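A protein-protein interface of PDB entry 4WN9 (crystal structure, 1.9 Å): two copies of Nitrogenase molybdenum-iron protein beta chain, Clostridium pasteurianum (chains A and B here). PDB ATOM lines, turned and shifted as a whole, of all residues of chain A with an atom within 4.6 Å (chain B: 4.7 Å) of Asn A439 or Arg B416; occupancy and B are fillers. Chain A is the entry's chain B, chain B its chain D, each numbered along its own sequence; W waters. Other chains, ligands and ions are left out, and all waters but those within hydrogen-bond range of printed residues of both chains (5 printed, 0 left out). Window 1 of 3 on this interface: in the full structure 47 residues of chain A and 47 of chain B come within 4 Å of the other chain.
No position is printed for both chains.
Of the 11 pairs that touch across the chains among the printed residues, none has its exchanged pair printed and touching as well.
The guanidinium group (NH2) of Arg B408 is in salt-bridge range of the side-chain carboxylate (OE2) of Glu A446.
The side-chain carboxylate of Asp A443 lies within salt-bridge range of the guanidinium group of Arg B416, 2.9 Å away.
OE2 of Glu A446 lies within salt-bridge range of NH1 of Arg B416.
Water W3 lies within hydrogen-bond range of the side-chain amide oxygen (OD1) of Asn A439 (2.6 Å), the side-chain hydroxyl (OG1) of Thr A438 (2.8 Å) and the backbone NH (N) of Tyr B417 (2.9 Å).
Water W4 lies within hydrogen-bond range of the backbone carbonyl oxygen of Gly B418 and the side-chain carboxylate of Glu A435.
Water W5 bridges OD1 of Asp A443 (2.8 Å) and NH1 of Arg B408 (2.9 Å).
Water W2 bridges OD1 of Asp A443 (2.8 Å) and NE of Arg B416 (3.0 Å).
Water W1 lies within hydrogen-bond range of OE2 of Glu A446 (3.0 Å) and NH2 of Arg B408 (3.2 Å).
Hydrophobic or aromatic side chains of chain A that line the printed part of chain B: Leu A442.
Hydrophobic or aromatic side chains of chain B within 4 Å of the printed part of chain A: Tyr B417 and His B419.
Along chain B the printed residues that touch a printed residue of chain A span positions 408 to 419.
Among the printed residues, Asp or Glu carboxylates within 4 Å of a Lys or Arg side-chain nitrogen of the other chain: Asp A443 with Arg B416, Glu A446 with Arg B408 and Glu A446 with Arg B416.
The guanidinium group (NH1) of Arg B416 is in salt-bridge range of the side-chain carboxylate (OD2) of Asp B415, at 3.9 Å.
The guanidinium group (NH2) of Arg B408 lies within salt-bridge range of the side-chain carboxylate (OD2) of Asp B415, 2.9 Å away.
The backbone NH (N) of Gly B418 is in hydrogen-bond range of the side-chain hydroxyl (OH) of Tyr B420, 3.3 Å away.
OG1 of Thr A438 lies within hydrogen-bond range of O of Glu A435 (3.3 Å).
The side-chain amide oxygen (OD1) of Asn A439 lies close to the backbone carbonyl oxygen (O) of Glu A435 (3.3 Å).
Among the printed residues, merely in contact across the chains: Glu A435 with Tyr B417 (3.4 Å), Glu A435 with Gly B418 (3.9 Å), Glu A435 with His B419 (3.4 Å), Thr A438 with Tyr B417 (3.98 Å), Asn A439 with Arg B416 (3.4 Å), Leu A442 with Asp B415 (3.8 Å), Leu A442 with Arg B416 (3.6 Å) and Glu A446 with Asp B415 (3.99 Å).
Of the printed residues of chain B, Glu A435 touches Tyr B417, Gly B418 and His B419.
Of the printed residues of chain B, Thr A438 touches Tyr B417 (3.98 Å).
Printed residues of chain B within 4 Å of Asn A439: Arg B416 (3.4 Å).
Ile A441 touches none of the printed residues of chain B.
Printed residues of chain B within 4 Å of Leu A442: Asp B415 (3.8 Å) and Arg B416 (3.6 Å).
Of the printed residues of chain A, Asp B415 touches Leu A442 (3.8 Å) and Glu A446 (3.99 Å).
Printed residues of chain A within 4 Å of His B419: Glu A435.
The nearest printed residue of chain A that does not touch Asp B415 is Asn A439 (6.2 Å).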
ATOM      1  N   GLU A 435     -15.182  15.036 -33.069  1.00  0.00           N
ATOM      2  CA  GLU A 435     -15.040  14.812 -31.639  1.00  0.00           C
ATOM      3  C   GLU A 435     -14.066  13.637 -31.373  1.00  0.00           C
ATOM      4  O   GLU A 435     -13.179  13.736 -30.542  1.00  0.00           O
ATOM      5  CB  GLU A 435     -16.380  14.524 -30.973  1.00  0.00           C
ATOM      6  CG  GLU A 435     -16.201  14.175 -29.493  1.00  0.00           C
ATOM      7  CD  GLU A 435     -17.490  13.798 -28.790  1.00  0.00           C
ATOM      8  OE1 GLU A 435     -18.412  13.260 -29.431  1.00  0.00           O
ATOM      9  OE2 GLU A 435     -17.558  14.053 -27.575  1.00  0.00           O
ATOM     10  N   GLU A 436     -14.211  12.555 -32.124  1.00  0.00           N
ATOM     11  CA  GLU A 436     -13.467  11.347 -31.872  1.00  0.00           C
ATOM     12  C   GLU A 436     -11.991  11.607 -32.222  1.00  0.00           C
ATOM     13  O   GLU A 436     -11.062  11.288 -31.444  1.00  0.00           O
ATOM     14  CB  GLU A 436     -14.064  10.181 -32.665  1.00  0.00           C
ATOM     15  CG  GLU A 436     -13.388   8.841 -32.412  1.00  0.00           C
ATOM     16  CD  GLU A 436     -14.125   7.662 -33.068  1.00  0.00           C
ATOM     17  OE1 GLU A 436     -15.019   7.886 -33.937  1.00  0.00           O
ATOM     18  OE2 GLU A 436     -13.797   6.499 -32.718  1.00  0.00           O
ATOM     19  N   ILE A 437     -11.773  12.250 -33.352  1.00  0.00           N
ATOM     20  CA  ILE A 437     -10.410  12.568 -33.766  1.00  0.00           C
ATOM     21  C   ILE A 437      -9.714  13.498 -32.762  1.00  0.00           C
ATOM     22  O   ILE A 437      -8.573  13.229 -32.358  1.00  0.00           O
ATOM     23  CB  ILE A 437     -10.362  13.222 -35.155  1.00  0.00           C
ATOM     24  CG1 ILE A 437     -10.681  12.191 -36.231  1.00  0.00           C
ATOM     25  CG2 ILE A 437      -8.987  13.848 -35.368  1.00  0.00           C
ATOM     26  CD1 ILE A 437     -11.078  12.781 -37.563  1.00  0.00           C
ATOM     27  N   THR A 438     -10.370  14.588 -32.360  1.00  0.00           N
ATOM     28  CA  THR A 438      -9.737  15.475 -31.394  1.00  0.00           C
ATOM     29  C   THR A 438      -9.584  14.822 -30.013  1.00  0.00           C
ATOM     30  O   THR A 438      -8.585  15.062 -29.331  1.00  0.00           O
ATOM     31  CB  THR A 438     -10.419  16.848 -31.291  1.00  0.00           C
ATOM     32  OG1 THR A 438     -11.808  16.676 -31.033  1.00  0.00           O
ATOM     33  CG2 THR A 438     -10.219  17.626 -32.568  1.00  0.00           C
ATOM     34  N   ASN A 439     -10.569  14.022 -29.589  1.00  0.00           N
ATOM     35  CA  ASN A 439     -10.452  13.313 -28.343  1.00  0.00           C
ATOM     36  C   ASN A 439      -9.198  12.455 -28.291  1.00  0.00           C
ATOM     37  O   ASN A 439      -8.522  12.429 -27.276  1.00  0.00           O
ATOM     38  CB  ASN A 439     -11.619  12.364 -28.104  1.00  0.00           C
ATOM     39  CG  ASN A 439     -12.857  13.034 -27.579  1.00  0.00           C
ATOM     40  OD1 ASN A 439     -12.914  14.241 -27.311  1.00  0.00           O
ATOM     41  ND2 ASN A 439     -13.883  12.215 -27.411  1.00  0.00           N
ATOM     42  N   VAL A 440      -8.957  11.648 -29.322  1.00  0.00           N
ATOM     43  CA  VAL A 440      -7.835  10.705 -29.255  1.00  0.00           C
ATOM     44  C   VAL A 440      -6.523  11.502 -29.310  1.00  0.00           C
ATOM     45  O   VAL A 440      -5.526  11.110 -28.702  1.00  0.00           O
ATOM     46  CB  VAL A 440      -7.851   9.564 -30.304  1.00  0.00           C
ATOM     47  CG1 VAL A 440      -9.047   8.627 -30.107  1.00  0.00           C
ATOM     48  CG2 VAL A 440      -7.762  10.097 -31.728  1.00  0.00           C
ATOM     49  N   ILE A 441      -6.559  12.646 -29.975  1.00  0.00           N
ATOM     50  CA  ILE A 441      -5.384  13.502 -30.099  1.00  0.00           C
ATOM     51  C   ILE A 441      -5.092  14.133 -28.741  1.00  0.00           C
ATOM     52  O   ILE A 441      -3.946  14.116 -28.287  1.00  0.00           O
ATOM     53  CB  ILE A 441      -5.560  14.581 -31.198  1.00  0.00           C
ATOM     54  CG1 ILE A 441      -5.329  13.964 -32.581  1.00  0.00           C
ATOM     55  CG2 ILE A 441      -4.549  15.696 -31.032  1.00  0.00           C
ATOM     56  CD1 ILE A 441      -5.747  14.824 -33.745  1.00  0.00           C
ATOM     57  N   LEU A 442      -6.138  14.602 -28.063  1.00  0.00           N
ATOM     58  CA  LEU A 442      -5.965  15.248 -26.770  1.00  0.00           C
ATOM     59  C   LEU A 442      -5.656  14.226 -25.684  1.00  0.00           C
ATOM     60  O   LEU A 442      -4.856  14.475 -24.799  1.00  0.00           O
ATOM     61  CB  LEU A 442      -7.192  16.076 -26.433  1.00  0.00           C
ATOM     62  CG  LEU A 442      -7.235  17.396 -27.200  1.00  0.00           C
ATOM     63  CD1 LEU A 442      -8.632  18.001 -27.149  1.00  0.00           C
ATOM     64  CD2 LEU A 442      -6.213  18.382 -26.662  1.00  0.00           C
ATOM     65  N   ASP A 443      -6.256  13.054 -25.764  1.00  0.00           N
ATOM     66  CA  ASP A 443      -5.909  12.007 -24.789  1.00  0.00           C
ATOM     67  C   ASP A 443      -4.400  11.758 -24.731  1.00  0.00           C
ATOM     68  O   ASP A 443      -3.822  11.658 -23.634  1.00  0.00           O
ATOM     69  CB  ASP A 443      -6.600  10.704 -25.112  1.00  0.00           C
ATOM     70  CG  ASP A 443      -8.064  10.661 -24.643  1.00  0.00           C
ATOM     71  OD1 ASP A 443      -8.494  11.468 -23.819  1.00  0.00           O
ATOM     72  OD2 ASP A 443      -8.779   9.776 -25.129  1.00  0.00           O
ATOM     73  N   GLU A 446      -2.345  14.734 -23.261  1.00  0.00           N
ATOM     74  CA  GLU A 446      -2.494  14.940 -21.839  1.00  0.00           C
ATOM     75  C   GLU A 446      -1.894  13.790 -21.059  1.00  0.00           C
ATOM     76  O   GLU A 446      -1.445  13.972 -19.931  1.00  0.00           O
ATOM     77  CB  GLU A 446      -3.965  15.164 -21.461  1.00  0.00           C
ATOM     78  CG  GLU A 446      -4.530  16.385 -22.141  1.00  0.00           C
ATOM     79  CD  GLU A 446      -5.750  16.971 -21.479  1.00  0.00           C
ATOM     80  OE1 GLU A 446      -5.712  18.189 -21.202  1.00  0.00           O
ATOM     81  OE2 GLU A 446      -6.739  16.242 -21.230  1.00  0.00           O
ATOM     82  N   LYS B  61     -17.621  26.310 -25.671  1.00  0.00           N
ATOM     83  CA  LYS B  61     -16.813  26.861 -26.768  1.00  0.00           C
ATOM     84  C   LYS B  61     -17.749  27.747 -27.572  1.00  0.00           C
ATOM     85  O   LYS B  61     -17.787  27.704 -28.796  1.00  0.00           O
ATOM     86  CB  LYS B  61     -16.164  25.783 -27.647  1.00  0.00           C
ATOM     87  CG  LYS B  61     -15.290  24.763 -26.923  1.00  0.00           C
ATOM     88  CD  LYS B  61     -14.221  25.399 -26.048  1.00  0.00           C
ATOM     89  CE  LYS B  61     -13.300  24.350 -25.446  1.00  0.00           C
ATOM     90  NZ  LYS B  61     -12.570  24.855 -24.252  1.00  0.00           N
ATOM     91  N   ARG B 408     -15.636  11.942 -18.918  1.00  0.00           N
ATOM     92  CA  ARG B 408     -16.042  13.299 -18.678  1.00  0.00           C
ATOM     93  C   ARG B 408     -17.553  13.369 -18.673  1.00  0.00           C
ATOM     94  O   ARG B 408     -18.201  12.886 -19.599  1.00  0.00           O
ATOM     95  CB  ARG B 408     -15.447  14.248 -19.721  1.00  0.00           C
ATOM     96  CG  ARG B 408     -13.947  14.417 -19.562  1.00  0.00           C
ATOM     97  CD  ARG B 408     -13.299  15.168 -20.732  1.00  0.00           C
ATOM     98  NE  ARG B 408     -11.927  15.512 -20.385  1.00  0.00           N
ATOM     99  CZ  ARG B 408     -10.923  14.650 -20.394  1.00  0.00           C
ATOM    100  NH1 ARG B 408     -11.111  13.369 -20.724  1.00  0.00           N
ATOM    101  NH2 ARG B 408      -9.720  15.059 -20.055  1.00  0.00           N
ATOM    102  N   MET B 414     -14.367  21.319 -19.968  1.00  0.00           N
ATOM    103  CA  MET B 414     -13.759  22.476 -20.609  1.00  0.00           C
ATOM    104  C   MET B 414     -12.563  22.094 -21.492  1.00  0.00           C
ATOM    105  O   MET B 414     -11.791  22.972 -21.940  1.00  0.00           O
ATOM    106  CB  MET B 414     -13.307  23.441 -19.530  1.00  0.00           C
ATOM    107  CG  MET B 414     -14.418  23.897 -18.599  1.00  0.00           C
ATOM    108  SD  MET B 414     -13.897  25.113 -17.404  1.00  0.00           S
ATOM    109  CE  MET B 414     -12.981  24.109 -16.246  1.00  0.00           C
ATOM    110  N   ASP B 415     -12.382  20.804 -21.743  1.00  0.00           N
ATOM    111  CA  ASP B 415     -11.129  20.360 -22.373  1.00  0.00           C
ATOM    112  C   ASP B 415     -11.269  19.406 -23.520  1.00  0.00           C
ATOM    113  O   ASP B 415     -10.315  18.719 -23.854  1.00  0.00           O
ATOM    114  CB  ASP B 415     -10.173  19.761 -21.329  1.00  0.00           C
ATOM    115  CG  ASP B 415     -10.818  18.675 -20.479  1.00  0.00           C
ATOM    116  OD1 ASP B 415     -12.061  18.511 -20.497  1.00  0.00           O
ATOM    117  OD2 ASP B 415     -10.042  17.964 -19.804  1.00  0.00           O
ATOM    118  N   ARG B 416     -12.463  19.370 -24.101  1.00  0.00           N
ATOM    119  CA  ARG B 416     -12.788  18.507 -25.243  1.00  0.00           C
ATOM    120  C   ARG B 416     -13.772  19.267 -26.159  1.00  0.00           C
ATOM    121  O   ARG B 416     -14.434  20.231 -25.749  1.00  0.00           O
ATOM    122  CB  ARG B 416     -13.381  17.157 -24.800  1.00  0.00           C
ATOM    123  CG  ARG B 416     -12.420  16.193 -24.081  1.00  0.00           C
ATOM    124  CD  ARG B 416     -11.203  15.893 -24.939  1.00  0.00           C
ATOM    125  NE  ARG B 416     -10.257  14.909 -24.398  1.00  0.00           N
ATOM    126  CZ  ARG B 416      -9.206  15.213 -23.633  1.00  0.00           C
ATOM    127  NH1 ARG B 416      -8.986  16.462 -23.238  1.00  0.00           N
ATOM    128  NH2 ARG B 416      -8.377  14.265 -23.240  1.00  0.00           N
ATOM    129  N   TYR B 417     -13.856  18.809 -27.395  1.00  0.00           N
ATOM    130  CA  TYR B 417     -14.617  19.486 -28.431  1.00  0.00           C
ATOM    131  C   TYR B 417     -15.714  18.600 -28.965  1.00  0.00           C
ATOM    132  O   TYR B 417     -15.472  17.490 -29.428  1.00  0.00           O
ATOM    133  CB  TYR B 417     -13.666  19.877 -29.565  1.00  0.00           C
ATOM    134  CG  TYR B 417     -12.722  20.967 -29.146  1.00  0.00           C
ATOM    135  CD1 TYR B 417     -11.510  20.675 -28.555  1.00  0.00           C
ATOM    136  CD2 TYR B 417     -13.074  22.296 -29.306  1.00  0.00           C
ATOM    137  CE1 TYR B 417     -10.696  21.681 -28.091  1.00  0.00           C
ATOM    138  CE2 TYR B 417     -12.255  23.312 -28.892  1.00  0.00           C
ATOM    139  CZ  TYR B 417     -11.062  23.007 -28.293  1.00  0.00           C
ATOM    140  OH  TYR B 417     -10.258  24.054 -27.885  1.00  0.00           O
ATOM    141  N   GLY B 418     -16.946  19.097 -28.895  1.00  0.00           N
ATOM    142  CA  GLY B 418     -18.082  18.413 -29.487  1.00  0.00           C
ATOM    143  C   GLY B 418     -18.876  17.598 -28.498  1.00  0.00           C
ATOM    144  O   GLY B 418     -19.927  17.079 -28.851  1.00  0.00           O
ATOM    145  N   HIS B 419     -18.410  17.518 -27.256  1.00  0.00           N
ATOM    146  CA  HIS B 419     -19.122  16.733 -26.230  1.00  0.00           C
ATOM    147  C   HIS B 419     -20.539  17.276 -25.968  1.00  0.00           C
ATOM    148  O   HIS B 419     -21.462  16.495 -25.704  1.00  0.00           O
ATOM    149  CB  HIS B 419     -18.300  16.672 -24.924  1.00  0.00           C
ATOM    150  CG  HIS B 419     -18.095  18.003 -24.272  1.00  0.00           C
ATOM    151  ND1 HIS B 419     -19.016  18.571 -23.423  1.00  0.00           N
ATOM    152  CD2 HIS B 419     -17.054  18.866 -24.324  1.00  0.00           C
ATOM    153  CE1 HIS B 419     -18.561  19.741 -23.006  1.00  0.00           C
ATOM    154  NE2 HIS B 419     -17.368  19.937 -23.541  1.00  0.00           N
ATOM    155  N   TYR B 420     -20.710  18.595 -26.110  1.00  0.00           N
ATOM    156  CA  TYR B 420     -21.980  19.275 -25.856  1.00  0.00           C
ATOM    157  C   TYR B 420     -23.054  19.012 -26.948  1.00  0.00           C
ATOM    158  O   TYR B 420     -24.184  19.529 -26.867  1.00  0.00           O
ATOM    159  CB  TYR B 420     -21.732  20.785 -25.669  1.00  0.00           C
ATOM    160  CG  TYR B 420     -20.584  21.258 -26.509  1.00  0.00           C
ATOM    161  CD1 TYR B 420     -20.752  21.462 -27.865  1.00  0.00           C
ATOM    162  CD2 TYR B 420     -19.332  21.444 -25.962  1.00  0.00           C
ATOM    163  CE1 TYR B 420     -19.700  21.821 -28.664  1.00  0.00           C
ATOM    164  CE2 TYR B 420     -18.259  21.820 -26.753  1.00  0.00           C
ATOM    165  CZ  TYR B 420     -18.456  22.007 -28.102  1.00  0.00           C
ATOM    166  OH  TYR B 420     -17.412  22.368 -28.920  1.00  0.00           O
HETATM  167  O   HOH W   1      -6.896  13.494 -20.091  1.00  0.00           O
HETATM  168  O   HOH W   2     -11.128  12.057 -24.693  1.00  0.00           O
HETATM  169  O   HOH W   3     -12.151  16.582 -28.282  1.00  0.00           O
HETATM  170  O   HOH W   4     -20.035  15.075 -30.734  1.00  0.00           O
HETATM  171  O   HOH W   5      -9.034  11.402 -21.116  1.00  0.00           O
